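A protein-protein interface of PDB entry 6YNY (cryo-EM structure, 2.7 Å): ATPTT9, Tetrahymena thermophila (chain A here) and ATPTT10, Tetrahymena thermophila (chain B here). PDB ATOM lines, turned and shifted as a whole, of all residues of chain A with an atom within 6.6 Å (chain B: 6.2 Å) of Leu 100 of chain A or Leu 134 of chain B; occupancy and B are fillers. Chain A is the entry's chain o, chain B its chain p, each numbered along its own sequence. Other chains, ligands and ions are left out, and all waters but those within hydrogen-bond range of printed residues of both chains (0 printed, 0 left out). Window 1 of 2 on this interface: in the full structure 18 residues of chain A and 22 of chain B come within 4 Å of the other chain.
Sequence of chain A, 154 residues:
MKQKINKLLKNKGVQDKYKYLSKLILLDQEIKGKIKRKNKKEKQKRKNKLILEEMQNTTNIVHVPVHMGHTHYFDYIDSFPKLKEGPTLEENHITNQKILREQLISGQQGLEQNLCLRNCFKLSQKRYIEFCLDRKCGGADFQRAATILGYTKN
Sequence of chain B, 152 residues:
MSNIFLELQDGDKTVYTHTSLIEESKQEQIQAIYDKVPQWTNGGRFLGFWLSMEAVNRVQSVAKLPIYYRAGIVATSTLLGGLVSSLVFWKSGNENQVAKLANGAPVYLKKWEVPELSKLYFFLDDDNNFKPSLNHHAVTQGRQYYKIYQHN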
ATOM      1  N   THR A  95      -0.386 -17.553  12.886  1.00  0.00           N
ATOM      2  CA  THR A  95       0.823 -18.291  13.226  1.00  0.00           C
ATOM      3  C   THR A  95       1.056 -19.441  12.259  1.00  0.00           C
ATOM      4  O   THR A  95       2.196 -19.715  11.868  1.00  0.00           O
ATOM      5  CB  THR A  95       0.727 -18.809  14.658  1.00  0.00           C
ATOM      6  OG1 THR A  95       0.756 -17.707  15.571  1.00  0.00           O
ATOM      7  CG2 THR A  95       1.863 -19.755  14.965  1.00  0.00           C
ATOM      8  N   ASN A  96      -0.014 -20.127  11.861  1.00  0.00           N
ATOM      9  CA  ASN A  96       0.119 -21.248  10.941  1.00  0.00           C
ATOM     10  C   ASN A  96       0.365 -20.782   9.512  1.00  0.00           C
ATOM     11  O   ASN A  96       1.107 -21.430   8.768  1.00  0.00           O
ATOM     12  CB  ASN A  96      -1.129 -22.123  11.008  1.00  0.00           C
ATOM     13  CG  ASN A  96      -1.346 -22.724  12.377  1.00  0.00           C
ATOM     14  OD1 ASN A  96      -0.414 -22.844  13.171  1.00  0.00           O
ATOM     15  ND2 ASN A  96      -2.579 -23.114  12.661  1.00  0.00           N
ATOM     16  N   GLN A  97      -0.243 -19.665   9.110  1.00  0.00           N
ATOM     17  CA  GLN A  97      -0.014 -19.151   7.764  1.00  0.00           C
ATOM     18  C   GLN A  97       1.462 -18.859   7.530  1.00  0.00           C
ATOM     19  O   GLN A  97       1.972 -19.051   6.421  1.00  0.00           O
ATOM     20  CB  GLN A  97      -0.844 -17.891   7.532  1.00  0.00           C
ATOM     21  CG  GLN A  97      -2.339 -18.117   7.526  1.00  0.00           C
ATOM     22  CD  GLN A  97      -2.806 -18.941   6.351  1.00  0.00           C
ATOM     23  OE1 GLN A  97      -2.981 -18.427   5.248  1.00  0.00           O
ATOM     24  NE2 GLN A  97      -3.010 -20.229   6.581  1.00  0.00           N
ATOM     25  N   LYS A  98       2.164 -18.393   8.563  1.00  0.00           N
ATOM     26  CA  LYS A  98       3.591 -18.125   8.423  1.00  0.00           C
ATOM     27  C   LYS A  98       4.377 -19.412   8.222  1.00  0.00           C
ATOM     28  O   LYS A  98       5.367 -19.434   7.482  1.00  0.00           O
ATOM     29  CB  LYS A  98       4.104 -17.375   9.647  1.00  0.00           C
ATOM     30  CG  LYS A  98       3.546 -15.977   9.793  1.00  0.00           C
ATOM     31  CD  LYS A  98       4.017 -15.311  11.074  1.00  0.00           C
ATOM     32  CE  LYS A  98       5.522 -15.098  11.077  1.00  0.00           C
ATOM     33  NZ  LYS A  98       5.983 -14.329  12.263  1.00  0.00           N
ATOM     34  N   ILE A  99       3.954 -20.493   8.876  1.00  0.00           N
ATOM     35  CA  ILE A  99       4.637 -21.770   8.718  1.00  0.00           C
ATOM     36  C   ILE A  99       4.340 -22.367   7.351  1.00  0.00           C
ATOM     37  O   ILE A  99       5.227 -22.927   6.697  1.00  0.00           O
ATOM     38  CB  ILE A  99       4.233 -22.727   9.852  1.00  0.00           C
ATOM     39  CG1 ILE A  99       4.590 -22.117  11.206  1.00  0.00           C
ATOM     40  CG2 ILE A  99       4.918 -24.063   9.685  1.00  0.00           C
ATOM     41  CD1 ILE A  99       4.057 -22.883  12.385  1.00  0.00           C
ATOM     42  N   LEU A 100       3.093 -22.259   6.894  1.00  0.00           N
ATOM     43  CA  LEU A 100       2.737 -22.802   5.591  1.00  0.00           C
ATOM     44  C   LEU A 100       3.326 -21.981   4.455  1.00  0.00           C
ATOM     45  O   LEU A 100       3.586 -22.520   3.374  1.00  0.00           O
ATOM     46  CB  LEU A 100       1.220 -22.875   5.454  1.00  0.00           C
ATOM     47  CG  LEU A 100       0.472 -23.681   6.511  1.00  0.00           C
ATOM     48  CD1 LEU A 100      -1.011 -23.587   6.261  1.00  0.00           C
ATOM     49  CD2 LEU A 100       0.915 -25.123   6.521  1.00  0.00           C
ATOM     50  N   ARG A 101       3.539 -20.683   4.672  1.00  0.00           N
ATOM     51  CA  ARG A 101       4.079 -19.840   3.613  1.00  0.00           C
ATOM     52  C   ARG A 101       5.544 -20.161   3.357  1.00  0.00           C
ATOM     53  O   ARG A 101       5.947 -20.406   2.214  1.00  0.00           O
ATOM     54  CB  ARG A 101       3.901 -18.369   3.977  1.00  0.00           C
ATOM     55  CG  ARG A 101       4.280 -17.423   2.865  1.00  0.00           C
ATOM     56  CD  ARG A 101       4.006 -15.976   3.210  1.00  0.00           C
ATOM     57  NE  ARG A 101       2.586 -15.719   3.436  1.00  0.00           N
ATOM     58  CZ  ARG A 101       2.030 -15.470   4.618  1.00  0.00           C
ATOM     59  NH1 ARG A 101       2.758 -15.423   5.723  1.00  0.00           N
ATOM     60  NH2 ARG A 101       0.728 -15.253   4.693  1.00  0.00           N
ATOM     61  N   GLU A 102       6.358 -20.162   4.411  1.00  0.00           N
ATOM     62  CA  GLU A 102       7.759 -20.537   4.262  1.00  0.00           C
ATOM     63  C   GLU A 102       7.886 -21.955   3.724  1.00  0.00           C
ATOM     64  O   GLU A 102       8.776 -22.247   2.916  1.00  0.00           O
ATOM     65  CB  GLU A 102       8.472 -20.402   5.606  1.00  0.00           C
ATOM     66  CG  GLU A 102       9.965 -20.684   5.571  1.00  0.00           C
ATOM     67  CD  GLU A 102      10.298 -22.163   5.664  1.00  0.00           C
ATOM     68  OE1 GLU A 102       9.380 -22.971   5.921  1.00  0.00           O
ATOM     69  OE2 GLU A 102      11.481 -22.518   5.480  1.00  0.00           O
ATOM     70  N   GLN A 103       7.001 -22.849   4.161  1.00  0.00           N
ATOM     71  CA  GLN A 103       7.017 -24.222   3.678  1.00  0.00           C
ATOM     72  C   GLN A 103       6.614 -24.308   2.214  1.00  0.00           C
ATOM     73  O   GLN A 103       6.999 -25.254   1.518  1.00  0.00           O
ATOM     74  CB  GLN A 103       6.083 -25.064   4.541  1.00  0.00           C
ATOM     75  CG  GLN A 103       6.177 -26.546   4.337  1.00  0.00           C
ATOM     76  CD  GLN A 103       5.241 -27.293   5.256  1.00  0.00           C
ATOM     77  OE1 GLN A 103       4.367 -26.697   5.880  1.00  0.00           O
ATOM     78  NE2 GLN A 103       5.419 -28.601   5.350  1.00  0.00           N
ATOM     79  N   LEU A 104       5.843 -23.335   1.731  1.00  0.00           N
ATOM     80  CA  LEU A 104       5.426 -23.324   0.335  1.00  0.00           C
ATOM     81  C   LEU A 104       6.515 -22.784  -0.578  1.00  0.00           C
ATOM     82  O   LEU A 104       6.618 -23.207  -1.735  1.00  0.00           O
ATOM     83  CB  LEU A 104       4.161 -22.480   0.183  1.00  0.00           C
ATOM     84  CG  LEU A 104       3.627 -22.248  -1.229  1.00  0.00           C
ATOM     85  CD1 LEU A 104       3.040 -23.518  -1.796  1.00  0.00           C
ATOM     86  CD2 LEU A 104       2.600 -21.146  -1.230  1.00  0.00           C
ATOM     87  N   ILE A 105       7.323 -21.853  -0.083  1.00  0.00           N
ATOM     88  CA  ILE A 105       8.323 -21.189  -0.907  1.00  0.00           C
ATOM     89  C   ILE A 105       9.673 -21.887  -0.823  1.00  0.00           C
ATOM     90  O   ILE A 105      10.351 -22.058  -1.838  1.00  0.00           O
ATOM     91  CB  ILE A 105       8.430 -19.711  -0.484  1.00  0.00           C
ATOM     92  CG1 ILE A 105       7.065 -19.034  -0.583  1.00  0.00           C
ATOM     93  CG2 ILE A 105       9.443 -18.981  -1.344  1.00  0.00           C
ATOM     94  CD1 ILE A 105       7.045 -17.631  -0.059  1.00  0.00           C
ATOM     95  N   GLN A 108       9.850 -27.038  -0.862  1.00  0.00           N
ATOM     96  CA  GLN A 108       9.291 -27.860  -1.922  1.00  0.00           C
ATOM     97  C   GLN A 108      10.336 -28.494  -2.826  1.00  0.00           C
ATOM     98  O   GLN A 108       9.982 -29.370  -3.622  1.00  0.00           O
ATOM     99  CB  GLN A 108       8.324 -27.035  -2.782  1.00  0.00           C
ATOM    100  CG  GLN A 108       7.075 -26.602  -2.045  1.00  0.00           C
ATOM    101  CD  GLN A 108       6.257 -27.772  -1.551  1.00  0.00           C
ATOM    102  OE1 GLN A 108       5.969 -28.704  -2.299  1.00  0.00           O
ATOM    103  NE2 GLN A 108       5.890 -27.740  -0.281  1.00  0.00           N
ATOM    104  N   LEU B 117      -3.553 -19.356   0.271  1.00  0.00           N
ATOM    105  CA  LEU B 117      -2.946 -20.047   1.399  1.00  0.00           C
ATOM    106  C   LEU B 117      -3.984 -20.452   2.433  1.00  0.00           C
ATOM    107  O   LEU B 117      -3.845 -21.497   3.078  1.00  0.00           O
ATOM    108  CB  LEU B 117      -1.884 -19.157   2.033  1.00  0.00           C
ATOM    109  CG  LEU B 117      -0.902 -19.828   2.984  1.00  0.00           C
ATOM    110  CD1 LEU B 117       0.006 -20.761   2.226  1.00  0.00           C
ATOM    111  CD2 LEU B 117      -0.098 -18.785   3.706  1.00  0.00           C
ATOM    112  N   LEU B 120      -5.671 -23.967   1.387  1.00  0.00           N
ATOM    113  CA  LEU B 120      -4.898 -25.180   1.178  1.00  0.00           C
ATOM    114  C   LEU B 120      -5.134 -26.174   2.304  1.00  0.00           C
ATOM    115  O   LEU B 120      -5.425 -25.801   3.444  1.00  0.00           O
ATOM    116  CB  LEU B 120      -3.410 -24.861   1.083  1.00  0.00           C
ATOM    117  CG  LEU B 120      -2.965 -24.082  -0.149  1.00  0.00           C
ATOM    118  CD1 LEU B 120      -1.512 -23.728  -0.031  1.00  0.00           C
ATOM    119  CD2 LEU B 120      -3.201 -24.888  -1.399  1.00  0.00           C
ATOM    120  N   TYR B 121      -4.999 -27.451   1.972  1.00  0.00           N
ATOM    121  CA  TYR B 121      -5.154 -28.520   2.943  1.00  0.00           C
ATOM    122  C   TYR B 121      -3.839 -28.748   3.669  1.00  0.00           C
ATOM    123  O   TYR B 121      -2.767 -28.742   3.057  1.00  0.00           O
ATOM    124  CB  TYR B 121      -5.605 -29.807   2.260  1.00  0.00           C
ATOM    125  CG  TYR B 121      -6.038 -30.889   3.213  1.00  0.00           C
ATOM    126  CD1 TYR B 121      -7.333 -30.929   3.695  1.00  0.00           C
ATOM    127  CD2 TYR B 121      -5.157 -31.872   3.625  1.00  0.00           C
ATOM    128  CE1 TYR B 121      -7.738 -31.913   4.562  1.00  0.00           C
ATOM    129  CE2 TYR B 121      -5.554 -32.862   4.494  1.00  0.00           C
ATOM    130  CZ  TYR B 121      -6.846 -32.878   4.959  1.00  0.00           C
ATOM    131  OH  TYR B 121      -7.247 -33.862   5.825  1.00  0.00           O
ATOM    132  N   PHE B 122      -3.928 -28.938   4.979  1.00  0.00           N
ATOM    133  CA  PHE B 122      -2.747 -29.160   5.792  1.00  0.00           C
ATOM    134  C   PHE B 122      -3.125 -30.045   6.966  1.00  0.00           C
ATOM    135  O   PHE B 122      -4.303 -30.246   7.271  1.00  0.00           O
ATOM    136  CB  PHE B 122      -2.137 -27.841   6.268  1.00  0.00           C
ATOM    137  CG  PHE B 122      -2.981 -27.099   7.258  1.00  0.00           C
ATOM    138  CD1 PHE B 122      -2.770 -27.250   8.612  1.00  0.00           C
ATOM    139  CD2 PHE B 122      -3.974 -26.241   6.837  1.00  0.00           C
ATOM    140  CE1 PHE B 122      -3.537 -26.568   9.522  1.00  0.00           C
ATOM    141  CE2 PHE B 122      -4.742 -25.557   7.746  1.00  0.00           C
ATOM    142  CZ  PHE B 122      -4.522 -25.719   9.087  1.00  0.00           C
ATOM    143  N   PHE B 123      -2.101 -30.584   7.620  1.00  0.00           N
ATOM    144  CA  PHE B 123      -2.288 -31.459   8.762  1.00  0.00           C
ATOM    145  C   PHE B 123      -1.241 -31.123   9.808  1.00  0.00           C
ATOM    146  O   PHE B 123      -0.256 -30.433   9.538  1.00  0.00           O
ATOM    147  CB  PHE B 123      -2.198 -32.931   8.355  1.00  0.00           C
ATOM    148  CG  PHE B 123      -0.798 -33.434   8.209  1.00  0.00           C
ATOM    149  CD1 PHE B 123       0.071 -32.854   7.308  1.00  0.00           C
ATOM    150  CD2 PHE B 123      -0.353 -34.499   8.962  1.00  0.00           C
ATOM    151  CE1 PHE B 123       1.352 -33.318   7.173  1.00  0.00           C
ATOM    152  CE2 PHE B 123       0.928 -34.967   8.829  1.00  0.00           C
ATOM    153  CZ  PHE B 123       1.782 -34.375   7.931  1.00  0.00           C
ATOM    154  N   PRO B 132       1.796 -27.397  11.686  1.00  0.00           N
ATOM    155  CA  PRO B 132       1.043 -27.532  10.438  1.00  0.00           C
ATOM    156  C   PRO B 132       1.969 -27.707   9.248  1.00  0.00           C
ATOM    157  O   PRO B 132       2.974 -27.007   9.108  1.00  0.00           O
ATOM    158  CB  PRO B 132       0.257 -26.220  10.355  1.00  0.00           C
ATOM    159  CG  PRO B 132       1.021 -25.272  11.175  1.00  0.00           C
ATOM    160  CD  PRO B 132       1.637 -26.060  12.277  1.00  0.00           C
ATOM    161  N   SER B 133       1.619 -28.656   8.384  1.00  0.00           N
ATOM    162  CA  SER B 133       2.445 -29.002   7.241  1.00  0.00           C
ATOM    163  C   SER B 133       1.579 -29.181   6.007  1.00  0.00           C
ATOM    164  O   SER B 133       0.485 -29.747   6.081  1.00  0.00           O
ATOM    165  CB  SER B 133       3.237 -30.283   7.505  1.00  0.00           C
ATOM    166  OG  SER B 133       4.021 -30.639   6.384  1.00  0.00           O
ATOM    167  N   LEU B 134       2.074 -28.687   4.874  1.00  0.00           N
ATOM    168  CA  LEU B 134       1.420 -28.923   3.597  1.00  0.00           C
ATOM    169  C   LEU B 134       1.740 -30.295   3.027  1.00  0.00           C
ATOM    170  O   LEU B 134       0.985 -30.795   2.187  1.00  0.00           O
ATOM    171  CB  LEU B 134       1.840 -27.858   2.589  1.00  0.00           C
ATOM    172  CG  LEU B 134       1.447 -26.416   2.889  1.00  0.00           C
ATOM    173  CD1 LEU B 134       2.125 -25.488   1.919  1.00  0.00           C
ATOM    174  CD2 LEU B 134      -0.047 -26.242   2.814  1.00  0.00           C
ATOM    175  N   ASN B 135       2.837 -30.911   3.464  1.00  0.00           N
ATOM    176  CA  ASN B 135       3.287 -32.191   2.926  1.00  0.00           C
ATOM    177  C   ASN B 135       2.529 -33.326   3.611  1.00  0.00           C
ATOM    178  O   ASN B 135       3.086 -34.151   4.338  1.00  0.00           O
ATOM    179  CB  ASN B 135       4.790 -32.338   3.104  1.00  0.00           C
ATOM    180  CG  ASN B 135       5.544 -31.067   2.777  1.00  0.00           C
ATOM    181  OD1 ASN B 135       6.382 -30.612   3.552  1.00  0.00           O
ATOM    182  ND2 ASN B 135       5.244 -30.482   1.628  1.00  0.00           N
ATOM    183  N   HIS B 136       1.224 -33.356   3.369  1.00  0.00           N
ATOM    184  CA  HIS B 136       0.395 -34.388   3.964  1.00  0.00           C
ATOM    185  C   HIS B 136       0.579 -35.710   3.225  1.00  0.00           C
ATOM    186  O   HIS B 136       1.146 -35.777   2.132  1.00  0.00           O
ATOM    187  CB  HIS B 136      -1.072 -33.966   3.982  1.00  0.00           C
ATOM    188  CG  HIS B 136      -1.605 -33.544   2.653  1.00  0.00           C
ATOM    189  ND1 HIS B 136      -2.049 -34.442   1.708  1.00  0.00           N
ATOM    190  CD2 HIS B 136      -1.777 -32.315   2.113  1.00  0.00           C
ATOM    191  CE1 HIS B 136      -2.466 -33.785   0.642  1.00  0.00           C
ATOM    192  NE2 HIS B 136      -2.311 -32.494   0.862  1.00  0.00           N
ATOM    193  N   VAL B 139       0.107 -36.195  -0.508  1.00  0.00           N
ATOM    194  CA  VAL B 139       0.894 -35.408  -1.447  1.00  0.00           C
ATOM    195  C   VAL B 139       1.779 -36.332  -2.268  1.00  0.00           C
ATOM    196  O   VAL B 139       2.229 -37.381  -1.795  1.00  0.00           O
ATOM    197  CB  VAL B 139       1.728 -34.356  -0.690  1.00  0.00           C
ATOM    198  CG1 VAL B 139       2.629 -33.611  -1.637  1.00  0.00           C
ATOM    199  CG2 VAL B 139       0.822 -33.399   0.031  1.00  0.00           C
ATOM    200  N   ARG B 143       4.755 -28.358  -5.305  1.00  0.00           N
ATOM    201  CA  ARG B 143       4.037 -27.160  -5.734  1.00  0.00           C
ATOM    202  C   ARG B 143       4.589 -26.581  -7.033  1.00  0.00           C
ATOM    203  O   ARG B 143       3.850 -26.419  -8.008  1.00  0.00           O
ATOM    204  CB  ARG B 143       4.090 -26.117  -4.614  1.00  0.00           C
ATOM    205  CG  ARG B 143       3.582 -26.640  -3.278  1.00  0.00           C
ATOM    206  CD  ARG B 143       2.084 -26.867  -3.284  1.00  0.00           C
ATOM    207  NE  ARG B 143       1.649 -27.626  -2.116  1.00  0.00           N
ATOM    208  CZ  ARG B 143       0.385 -27.928  -1.847  1.00  0.00           C
ATOM    209  NH1 ARG B 143      -0.587 -27.534  -2.659  1.00  0.00           N
ATOM    210  NH2 ARG B 143       0.092 -28.627  -0.761  1.00  0.00           N
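N of Asn 135 of chain B sits at hydrogen-bond distance from OG of Ser 133 of chain B, at 3.2 Å. The side-chain amide nitrogen (NE2) of Gln 108 of chain A is in hydrogen-bond range of the backbone carbonyl oxygen (O) of Gln 103 of chain A, 3.3 Å away. The backbone carbonyl oxygen (O) of Phe 123 of chain B is in hydrogen-bond range of the backbone NH (N) of Ser 133 of chain B (2.8 Å).
OE1 of Gln 103 of chain A sits at hydrogen-bond distance from N of Leu 134 of chain B, at 3.2 Å. The side-chain amide nitrogen (NE2) of Gln 103 of chain A lies within hydrogen-bond range of the side-chain amide oxygen (OD1) of Asn 135 of chain B, at 2.9 Å. The backbone NH of Arg 143 of chain B sits at hydrogen-bond distance from the side-chain amide oxygen of Gln 108 of chain A. The side-chain amide nitrogen of Gln 108 of chain A sits close to the side-chain amide nitrogen of Asn 135 of chain B. OG of Ser 133 of chain B sits at hydrogen-bond distance from NE2 of Gln 103 of chain A, 2.7 Å away.
Printed residues of chain B that touch a printed residue of chain A: Leu 117, Pro 132, Ser 133, Leu 134, Asn 135 and Arg 143. Along chain B the printed residues that touch a printed residue of chain A span positions 117 to 143. Hydrophobic or aromatic side chains of chain A within 4 Å of the printed part of chain B: Ile 99, Leu 100 and Leu 104. Among the printed residues, 13 pairs touch across the chains.
Of the printed residues of chain B, Leu 100 of chain A touches Pro 132 (3.8 Å) and Leu 134 (3.6 Å). Of the printed residues of chain B, Leu 104 of chain A touches Arg 143 (3.5 Å). Of the printed residues of chain B, Gln 108 of chain A touches Asn 135 and Arg 143. Tyr 121 of chain B touches none of the printed residues of chain A. Phe 123 of chain B touches none of the printed residues of chain A. Leu 134 of chain B touches two residues of chain A. The nearest printed residue of chain B that does not touch Leu 100 of chain A is Phe 122 of chain B (4.02 Å). The nearest residue of chain A that does not touch Leu 134 of chain B is Leu 104 of chain A (4.03 Å).
Asn 96 of chain A touches Pro 132 of chain B. CD2 of Leu 117 of chain B touches OE1 of Gln 97 of chain A, 3.3 Å away. Pro 132 of chain B touches Ile 99 of chain A (O to CG2, 3.6 Å). Leu 100 of chain A touches Pro 132 of chain B. O of Leu 100 of chain A touches CD1 of Leu 134 of chain B, 3.6 Å away. Arg 101 of chain A touches Leu 117 of chain B. O of Pro 132 of chain B touches OE1 of Gln 103 of chain A, at 3.5 Å. Leu 104 of chain A touches Arg 143 of chain B (CD1 to CG, 3.5 Å).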
